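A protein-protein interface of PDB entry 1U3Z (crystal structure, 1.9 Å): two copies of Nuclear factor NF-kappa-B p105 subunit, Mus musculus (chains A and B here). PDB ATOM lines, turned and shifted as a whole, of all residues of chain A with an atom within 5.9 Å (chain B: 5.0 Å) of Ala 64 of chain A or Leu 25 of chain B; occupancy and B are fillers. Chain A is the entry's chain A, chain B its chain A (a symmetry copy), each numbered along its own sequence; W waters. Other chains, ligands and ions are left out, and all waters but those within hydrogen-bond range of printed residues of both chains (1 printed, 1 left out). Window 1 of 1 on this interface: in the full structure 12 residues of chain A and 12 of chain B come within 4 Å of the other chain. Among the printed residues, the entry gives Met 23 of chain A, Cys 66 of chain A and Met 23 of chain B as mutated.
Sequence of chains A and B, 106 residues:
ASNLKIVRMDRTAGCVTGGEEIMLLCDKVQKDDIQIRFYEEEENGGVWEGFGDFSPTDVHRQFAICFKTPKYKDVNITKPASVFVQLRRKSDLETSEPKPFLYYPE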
ATOM      1  N   MET A  23       8.184  -8.542 -26.864  1.00  0.00           N
ATOM      2  CA  MET A  23       7.890  -9.930 -27.168  1.00  0.00           C
ATOM      3  C   MET A  23       6.372 -10.051 -27.244  1.00  0.00           C
ATOM      4  O   MET A  23       5.656  -9.624 -26.317  1.00  0.00           O
ATOM      5  CB  MET A  23       8.473 -10.821 -26.097  1.00  0.00           C
ATOM      6  CG  MET A  23       8.526 -12.311 -26.482  1.00  0.00           C
ATOM      7  SD  MET A  23       9.232 -13.370 -25.168  1.00  0.00           S
ATOM      8  CE  MET A  23      10.905 -13.262 -25.464  1.00  0.00           C
ATOM      9  N   LEU A  24       5.911 -10.633 -28.344  1.00  0.00           N
ATOM     10  CA  LEU A  24       4.500 -10.739 -28.704  1.00  0.00           C
ATOM     11  C   LEU A  24       4.123 -12.225 -28.970  1.00  0.00           C
ATOM     12  O   LEU A  24       4.802 -12.955 -29.684  1.00  0.00           O
ATOM     13  CB  LEU A  24       4.287  -9.839 -29.932  1.00  0.00           C
ATOM     14  CG  LEU A  24       2.941  -9.767 -30.618  1.00  0.00           C
ATOM     15  CD1 LEU A  24       2.772  -8.399 -31.308  1.00  0.00           C
ATOM     16  CD2 LEU A  24       2.682 -10.934 -31.543  1.00  0.00           C
ATOM     17  N   LEU A  25       3.030 -12.677 -28.378  1.00  0.00           N
ATOM     18  CA  LEU A  25       2.482 -13.996 -28.695  1.00  0.00           C
ATOM     19  C   LEU A  25       1.294 -13.824 -29.620  1.00  0.00           C
ATOM     20  O   LEU A  25       0.444 -12.993 -29.366  1.00  0.00           O
ATOM     21  CB  LEU A  25       2.059 -14.699 -27.459  1.00  0.00           C
ATOM     22  CG  LEU A  25       3.115 -14.722 -26.330  1.00  0.00           C
ATOM     23  CD1 LEU A  25       2.549 -15.393 -25.077  1.00  0.00           C
ATOM     24  CD2 LEU A  25       4.332 -15.378 -26.842  1.00  0.00           C
ATOM     25  N   CYS A  26       1.265 -14.614 -30.683  1.00  0.00           N
ATOM     26  CA  CYS A  26       0.235 -14.494 -31.714  1.00  0.00           C
ATOM     27  C   CYS A  26      -0.338 -15.873 -32.036  1.00  0.00           C
ATOM     28  O   CYS A  26       0.311 -16.881 -31.783  1.00  0.00           O
ATOM     29  CB  CYS A  26       0.860 -13.858 -32.974  1.00  0.00           C
ATOM     30  SG  CYS A  26       2.359 -14.597 -33.621  1.00  0.00           S
ATOM     31  N   VAL A  29       1.177 -17.450 -37.634  1.00  0.00           N
ATOM     32  CA  VAL A  29       1.555 -16.567 -38.732  1.00  0.00           C
ATOM     33  C   VAL A  29       2.633 -17.259 -39.560  1.00  0.00           C
ATOM     34  O   VAL A  29       3.225 -18.253 -39.118  1.00  0.00           O
ATOM     35  CB  VAL A  29       2.100 -15.193 -38.258  1.00  0.00           C
ATOM     36  CG1 VAL A  29       1.081 -14.469 -37.440  1.00  0.00           C
ATOM     37  CG2 VAL A  29       3.427 -15.338 -37.479  1.00  0.00           C
ATOM     38  N   ASP A  58      13.212 -13.712 -36.386  1.00  0.00           N
ATOM     39  CA  ASP A  58      12.672 -13.258 -35.089  1.00  0.00           C
ATOM     40  C   ASP A  58      11.261 -13.788 -34.788  1.00  0.00           C
ATOM     41  O   ASP A  58      10.689 -13.581 -33.684  1.00  0.00           O
ATOM     42  CB  ASP A  58      12.668 -11.736 -35.075  1.00  0.00           C
ATOM     43  CG  ASP A  58      14.048 -11.144 -35.151  1.00  0.00           C
ATOM     44  OD1 ASP A  58      14.925 -11.672 -34.481  1.00  0.00           O
ATOM     45  OD2 ASP A  58      14.351 -10.115 -35.790  1.00  0.00           O
ATOM     46  N   VAL A  59      10.692 -14.504 -35.750  1.00  0.00           N
ATOM     47  CA  VAL A  59       9.410 -15.142 -35.582  1.00  0.00           C
ATOM     48  C   VAL A  59       9.648 -16.558 -35.077  1.00  0.00           C
ATOM     49  O   VAL A  59      10.356 -17.354 -35.724  1.00  0.00           O
ATOM     50  CB  VAL A  59       8.600 -15.144 -36.908  1.00  0.00           C
ATOM     51  CG1 VAL A  59       7.224 -15.808 -36.700  1.00  0.00           C
ATOM     52  CG2 VAL A  59       8.496 -13.724 -37.462  1.00  0.00           C
ATOM     53  N   HIS A  60       9.084 -16.851 -33.909  1.00  0.00           N
ATOM     54  CA  HIS A  60       9.401 -18.059 -33.171  1.00  0.00           C
ATOM     55  C   HIS A  60       8.343 -19.076 -33.441  1.00  0.00           C
ATOM     56  O   HIS A  60       7.228 -18.993 -32.890  1.00  0.00           O
ATOM     57  CB  HIS A  60       9.505 -17.774 -31.665  1.00  0.00           C
ATOM     58  CG  HIS A  60       9.575 -18.999 -30.821  1.00  0.00           C
ATOM     59  ND1 HIS A  60      10.605 -19.907 -30.927  1.00  0.00           N
ATOM     60  CD2 HIS A  60       8.751 -19.468 -29.854  1.00  0.00           C
ATOM     61  CE1 HIS A  60      10.409 -20.887 -30.064  1.00  0.00           C
ATOM     62  NE2 HIS A  60       9.297 -20.641 -29.387  1.00  0.00           N
ATOM     63  N   ARG A  61       8.688 -20.030 -34.306  1.00  0.00           N
ATOM     64  CA  ARG A  61       7.853 -21.189 -34.613  1.00  0.00           C
ATOM     65  C   ARG A  61       6.428 -20.795 -34.974  1.00  0.00           C
ATOM     66  O   ARG A  61       5.488 -21.482 -34.568  1.00  0.00           O
ATOM     67  CB  ARG A  61       7.790 -22.123 -33.410  1.00  0.00           C
ATOM     68  CG  ARG A  61       9.113 -22.343 -32.785  1.00  0.00           C
ATOM     69  CD  ARG A  61      10.091 -23.016 -33.698  1.00  0.00           C
ATOM     70  NE  ARG A  61       9.708 -24.407 -33.848  1.00  0.00           N
ATOM     71  CZ  ARG A  61       9.147 -24.931 -34.929  1.00  0.00           C
ATOM     72  NH1 ARG A  61       8.877 -24.191 -35.996  1.00  0.00           N
ATOM     73  NH2 ARG A  61       8.845 -26.223 -34.928  1.00  0.00           N
ATOM     74  N   GLN A  62       6.298 -19.678 -35.683  1.00  0.00           N
ATOM     75  CA  GLN A  62       5.001 -19.158 -36.137  1.00  0.00           C
ATOM     76  C   GLN A  62       4.017 -18.684 -35.072  1.00  0.00           C
ATOM     77  O   GLN A  62       2.878 -18.325 -35.396  1.00  0.00           O
ATOM     78  CB  GLN A  62       4.312 -20.241 -36.980  1.00  0.00           C
ATOM     79  CG  GLN A  62       5.151 -20.699 -38.095  1.00  0.00           C
ATOM     80  CD  GLN A  62       4.405 -21.656 -38.978  1.00  0.00           C
ATOM     81  OE1 GLN A  62       4.121 -21.330 -40.125  1.00  0.00           O
ATOM     82  NE2 GLN A  62       4.036 -22.819 -38.430  1.00  0.00           N
ATOM     83  N   PHE A  63       4.422 -18.660 -33.811  1.00  0.00           N
ATOM     84  CA  PHE A  63       3.502 -18.338 -32.714  1.00  0.00           C
ATOM     85  C   PHE A  63       3.970 -17.206 -31.789  1.00  0.00           C
ATOM     86  O   PHE A  63       3.302 -16.910 -30.786  1.00  0.00           O
ATOM     87  CB  PHE A  63       3.245 -19.599 -31.898  1.00  0.00           C
ATOM     88  CG  PHE A  63       2.300 -20.576 -32.579  1.00  0.00           C
ATOM     89  CD1 PHE A  63       0.954 -20.262 -32.721  1.00  0.00           C
ATOM     90  CD2 PHE A  63       2.755 -21.830 -33.021  1.00  0.00           C
ATOM     91  CE1 PHE A  63       0.058 -21.167 -33.336  1.00  0.00           C
ATOM     92  CE2 PHE A  63       1.861 -22.752 -33.630  1.00  0.00           C
ATOM     93  CZ  PHE A  63       0.532 -22.421 -33.786  1.00  0.00           C
ATOM     94  N   ALA A  64       5.117 -16.621 -32.089  1.00  0.00           N
ATOM     95  CA  ALA A  64       5.589 -15.448 -31.354  1.00  0.00           C
ATOM     96  C   ALA A  64       6.503 -14.648 -32.203  1.00  0.00           C
ATOM     97  O   ALA A  64       7.071 -15.163 -33.148  1.00  0.00           O
ATOM     98  CB  ALA A  64       6.298 -15.824 -30.010  1.00  0.00           C
ATOM     99  N   ILE A  65       6.643 -13.364 -31.869  1.00  0.00           N
ATOM    100  CA  ILE A  65       7.534 -12.480 -32.570  1.00  0.00           C
ATOM    101  C   ILE A  65       8.223 -11.597 -31.575  1.00  0.00           C
ATOM    102  O   ILE A  65       7.573 -10.996 -30.687  1.00  0.00           O
ATOM    103  CB  ILE A  65       6.772 -11.568 -33.596  1.00  0.00           C
ATOM    104  CG1 ILE A  65       5.852 -12.402 -34.524  1.00  0.00           C
ATOM    105  CG2 ILE A  65       7.738 -10.661 -34.327  1.00  0.00           C
ATOM    106  CD1 ILE A  65       4.990 -11.545 -35.451  1.00  0.00           C
ATOM    107  N   CYS A  66       9.548 -11.495 -31.726  1.00  0.00           N
ATOM    108  CA  CYS A  66      10.350 -10.512 -31.040  1.00  0.00           C
ATOM    109  C   CYS A  66      10.670  -9.409 -32.019  1.00  0.00           C
ATOM    110  O   CYS A  66      11.098  -9.697 -33.158  1.00  0.00           O
ATOM    111  CB  CYS A  66      11.670 -11.147 -30.553  1.00  0.00           C
ATOM    112  SG  CYS A  66      11.366 -12.337 -29.225  1.00  0.00           S
ATOM    113  N   LYS B   5      14.215 -26.787 -24.823  1.00  0.00           N
ATOM    114  CA  LYS B   5      15.086 -25.678 -25.052  1.00  0.00           C
ATOM    115  C   LYS B   5      14.388 -24.363 -24.702  1.00  0.00           C
ATOM    116  O   LYS B   5      13.263 -24.154 -25.122  1.00  0.00           O
ATOM    117  CB  LYS B   5      15.556 -25.654 -26.494  1.00  0.00           C
ATOM    118  CG  LYS B   5      16.579 -24.576 -26.758  1.00  0.00           C
ATOM    119  CD  LYS B   5      17.046 -24.616 -28.202  1.00  0.00           C
ATOM    120  CE  LYS B   5      17.878 -23.383 -28.554  1.00  0.00           C
ATOM    121  NZ  LYS B   5      19.287 -23.472 -28.052  1.00  0.00           N
ATOM    122  N   ILE B   6      15.048 -23.555 -23.879  1.00  0.00           N
ATOM    123  CA  ILE B   6      14.683 -22.156 -23.652  1.00  0.00           C
ATOM    124  C   ILE B   6      15.332 -21.362 -24.790  1.00  0.00           C
ATOM    125  O   ILE B   6      16.562 -21.214 -24.857  1.00  0.00           O
ATOM    126  CB  ILE B   6      15.124 -21.600 -22.280  1.00  0.00           C
ATOM    127  CG1 ILE B   6      14.514 -22.448 -21.176  1.00  0.00           C
ATOM    128  CG2 ILE B   6      14.674 -20.117 -22.138  1.00  0.00           C
ATOM    129  CD1 ILE B   6      14.902 -22.110 -19.734  1.00  0.00           C
ATOM    130  N   VAL B   7      14.489 -20.898 -25.706  1.00  0.00           N
ATOM    131  CA  VAL B   7      14.970 -20.134 -26.871  1.00  0.00           C
ATOM    132  C   VAL B   7      15.243 -18.679 -26.487  1.00  0.00           C
ATOM    133  O   VAL B   7      16.267 -18.119 -26.843  1.00  0.00           O
ATOM    134  CB  VAL B   7      13.991 -20.289 -28.025  1.00  0.00           C
ATOM    135  CG1 VAL B   7      14.371 -19.383 -29.197  1.00  0.00           C
ATOM    136  CG2 VAL B   7      13.957 -21.746 -28.460  1.00  0.00           C
ATOM    137  N   ARG B   8      14.329 -18.055 -25.741  1.00  0.00           N
ATOM    138  CA  ARG B   8      14.548 -16.696 -25.285  1.00  0.00           C
ATOM    139  C   ARG B   8      13.671 -16.396 -24.102  1.00  0.00           C
ATOM    140  O   ARG B   8      12.611 -16.950 -23.972  1.00  0.00           O
ATOM    141  CB  ARG B   8      14.195 -15.731 -26.418  1.00  0.00           C
ATOM    142  CG  ARG B   8      14.802 -14.380 -26.251  1.00  0.00           C
ATOM    143  CD  ARG B   8      14.654 -13.509 -27.485  1.00  0.00           C
ATOM    144  NE  ARG B   8      15.038 -12.123 -27.209  1.00  0.00           N
ATOM    145  CZ  ARG B   8      15.241 -11.179 -28.120  1.00  0.00           C
ATOM    146  NH1 ARG B   8      15.575  -9.946 -27.722  1.00  0.00           N
ATOM    147  NH2 ARG B   8      15.123 -11.455 -29.420  1.00  0.00           N
ATOM    148  N   MET B   9      14.135 -15.525 -23.224  1.00  0.00           N
ATOM    149  CA  MET B   9      13.353 -15.012 -22.115  1.00  0.00           C
ATOM    150  C   MET B   9      13.389 -13.529 -22.224  1.00  0.00           C
ATOM    151  O   MET B   9      14.429 -12.951 -22.524  1.00  0.00           O
ATOM    152  CB  MET B   9      13.967 -15.419 -20.766  1.00  0.00           C
ATOM    153  CG  MET B   9      13.707 -16.894 -20.451  1.00  0.00           C
ATOM    154  SD  MET B   9      14.750 -17.460 -19.035  1.00  0.00           S
ATOM    155  CE  MET B   9      13.766 -16.851 -17.783  1.00  0.00           C
ATOM    156  N   MET B  23       8.056 -13.690 -19.826  1.00  0.00           N
ATOM    157  CA  MET B  23       7.605 -14.353 -21.035  1.00  0.00           C
ATOM    158  C   MET B  23       8.807 -15.101 -21.601  1.00  0.00           C
ATOM    159  O   MET B  23       9.892 -14.513 -21.779  1.00  0.00           O
ATOM    160  CB  MET B  23       7.070 -13.329 -22.008  1.00  0.00           C
ATOM    161  CG  MET B  23       6.256 -13.932 -23.168  1.00  0.00           C
ATOM    162  SD  MET B  23       5.623 -12.673 -24.335  1.00  0.00           S
ATOM    163  CE  MET B  23       4.165 -12.188 -23.601  1.00  0.00           C
ATOM    164  N   LEU B  24       8.591 -16.381 -21.875  1.00  0.00           N
ATOM    165  CA  LEU B  24       9.618 -17.330 -22.294  1.00  0.00           C
ATOM    166  C   LEU B  24       9.207 -18.015 -23.629  1.00  0.00           C
ATOM    167  O   LEU B  24       8.090 -18.489 -23.805  1.00  0.00           O
ATOM    168  CB  LEU B  24       9.795 -18.330 -21.140  1.00  0.00           C
ATOM    169  CG  LEU B  24      10.741 -19.504 -21.267  1.00  0.00           C
ATOM    170  CD1 LEU B  24      11.256 -19.920 -19.875  1.00  0.00           C
ATOM    171  CD2 LEU B  24      10.157 -20.655 -22.053  1.00  0.00           C
ATOM    172  N   LEU B  25      10.121 -18.055 -24.585  1.00  0.00           N
ATOM    173  CA  LEU B  25       9.909 -18.825 -25.810  1.00  0.00           C
ATOM    174  C   LEU B  25      10.689 -20.122 -25.715  1.00  0.00           C
ATOM    175  O   LEU B  25      11.847 -20.106 -25.344  1.00  0.00           O
ATOM    176  CB  LEU B  25      10.356 -18.056 -26.997  1.00  0.00           C
ATOM    177  CG  LEU B  25       9.818 -16.609 -27.074  1.00  0.00           C
ATOM    178  CD1 LEU B  25      10.405 -15.881 -28.286  1.00  0.00           C
ATOM    179  CD2 LEU B  25       8.344 -16.658 -27.083  1.00  0.00           C
ATOM    180  N   CYS B  26      10.030 -21.222 -26.047  1.00  0.00           N
ATOM    181  CA  CYS B  26      10.620 -22.553 -25.909  1.00  0.00           C
ATOM    182  C   CYS B  26      10.402 -23.351 -27.194  1.00  0.00           C
ATOM    183  O   CYS B  26       9.499 -23.041 -27.963  1.00  0.00           O
ATOM    184  CB  CYS B  26       9.966 -23.269 -24.709  1.00  0.00           C
ATOM    185  SG  CYS B  26       8.176 -23.331 -24.653  1.00  0.00           S
ATOM    186  N   ASP B  27      11.193 -24.396 -27.421  1.00  0.00           N
ATOM    187  CA  ASP B  27      10.767 -25.427 -28.377  1.00  0.00           C
ATOM    188  C   ASP B  27       9.537 -26.144 -27.840  1.00  0.00           C
ATOM    189  O   ASP B  27       9.105 -25.894 -26.722  1.00  0.00           O
ATOM    190  CB  ASP B  27      11.885 -26.416 -28.652  1.00  0.00           C
ATOM    191  CG  ASP B  27      12.966 -25.818 -29.495  1.00  0.00           C
ATOM    192  OD1 ASP B  27      14.067 -26.406 -29.531  1.00  0.00           O
ATOM    193  OD2 ASP B  27      12.800 -24.768 -30.147  1.00  0.00           O
ATOM    194  N   PHE B  63       4.616 -23.386 -27.502  1.00  0.00           N
ATOM    195  CA  PHE B  63       5.882 -22.757 -27.898  1.00  0.00           C
ATOM    196  C   PHE B  63       6.274 -21.522 -27.076  1.00  0.00           C
ATOM    197  O   PHE B  63       7.286 -20.872 -27.380  1.00  0.00           O
ATOM    198  CB  PHE B  63       5.813 -22.394 -29.376  1.00  0.00           C
ATOM    199  CG  PHE B  63       5.968 -23.591 -30.299  1.00  0.00           C
ATOM    200  CD1 PHE B  63       7.192 -24.239 -30.404  1.00  0.00           C
ATOM    201  CD2 PHE B  63       4.899 -24.024 -31.103  1.00  0.00           C
ATOM    202  CE1 PHE B  63       7.358 -25.343 -31.272  1.00  0.00           C
ATOM    203  CE2 PHE B  63       5.057 -25.126 -31.987  1.00  0.00           C
ATOM    204  CZ  PHE B  63       6.270 -25.776 -32.067  1.00  0.00           C
ATOM    205  N   ALA B  64       5.466 -21.176 -26.089  1.00  0.00           N
ATOM    206  CA  ALA B  64       5.812 -20.098 -25.162  1.00  0.00           C
ATOM    207  C   ALA B  64       5.117 -20.295 -23.869  1.00  0.00           C
ATOM    208  O   ALA B  64       4.113 -20.981 -23.809  1.00  0.00           O
ATOM    209  CB  ALA B  64       5.481 -18.681 -25.738  1.00  0.00           C
HETATM  210  O   HOH W   1      14.039 -13.689 -31.158  1.00  0.00           O
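Hydrophobic or aromatic side chains of chain A within 4 Å of the printed part of chain B: Met 23, Leu 25, His 60, Phe 63 and Ala 64.
Of the printed residues of chain B, Met 23 of chain A touches Met 23 and Leu 25.
Asp 58 of chain A touches none of the printed residues of chain B.
Ala 64 of chain A touches just one residue of chain B: Leu 25 (3.7 Å).
Of the printed residues of chain A, Arg 8 of chain B touches Cys 66.
Leu 24 of chain B touches none of the printed residues of chain A.
Leu 25 of chain B touches just these residues of chain A: Met 23 (3.8 Å), His 60 (3.6 Å), Ala 64 (3.7 Å) and Cys 66 (3.8 Å).
Of the printed residues of chain A, Ala 64 of chain B touches Leu 25.
The nearest printed residue of chain A that does not touch Met 23 of chain B is Leu 24 of chain A (4.5 Å).
A ring nitrogen (NE2) of His 60 of chain A sits at hydrogen-bond distance from the backbone carbonyl oxygen of Cys 26 of chain B, at 2.8 Å.
A ring nitrogen (NE2) of His 60 of chain A is in hydrogen-bond range of the backbone carbonyl oxygen of Phe 63 of chain B, 2.9 Å away.
The backbone carbonyl oxygen (O) of Met 23 of chain A lies close to the side-chain sulfur (SD) of Met 23 of chain B (3.6 Å).
Among the printed residues, merely in contact across the chains: His 60 of chain A with Leu 25 of chain B (3.6 Å), Arg 61 of chain A with Phe 63 of chain B (3.6 Å), Phe 63 of chain A with Phe 63 of chain B (3.6 Å), Cys 66 of chain A with Arg 8 of chain B (3.6 Å), Leu 25 of chain A with Ala 64 of chain B (3.7 Å), Ala 64 of chain A with Leu 25 of chain B (3.7 Å), Cys 66 of chain A with Leu 25 of chain B (3.8 Å), Met 23 of chain A with Leu 25 of chain B (3.8 Å), Leu 25 of chain A with Met 23 of chain B (3.8 Å) and His 60 of chain A with Val 7 of chain B (3.99 Å).
Water W1 lies within hydrogen-bond range of the guanidinium group of Arg 8 of chain B (3.0 Å) and the side-chain sulfur of Cys 66 of chain A (3.6 Å).
Met 23 of chain A touches its own counterpart, Met 23 of chain B.
Met 23 of chain A touches Leu 25 of chain B, and with the chains exchanged Leu 25 of chain A touches Met 23 of chain B.
Leu 25 of chain A touches Ala 64 of chain B, and with the chains exchanged Ala 64 of chain A touches Leu 25 of chain B.
Phe 63 of chain B touches its own counterpart, Phe 63 of chain A.
N of Cys 26 of chain A sits at hydrogen-bond distance from O of Phe 63 of chain A, at 3.1 Å.
The side-chain sulfur (SG) of Cys 26 of chain A is in hydrogen-bond range of the backbone NH (N) of Ala 64 of chain A, at 3.7 Å.
O of Asp 58 of chain A sits at hydrogen-bond distance from N of Cys 66 of chain A, at 3.1 Å.
The backbone NH (N) of Leu 25 of chain B lies within hydrogen-bond range of the backbone carbonyl oxygen (O) of Arg 8 of chain B, 2.8 Å away.
N of Cys 26 of chain B is in hydrogen-bond range of O of Phe 63 of chain B (3.1 Å).
The side-chain sulfur of Cys 26 of chain B is in hydrogen-bond range of the backbone NH of Ala 64 of chain B (3.7 Å).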
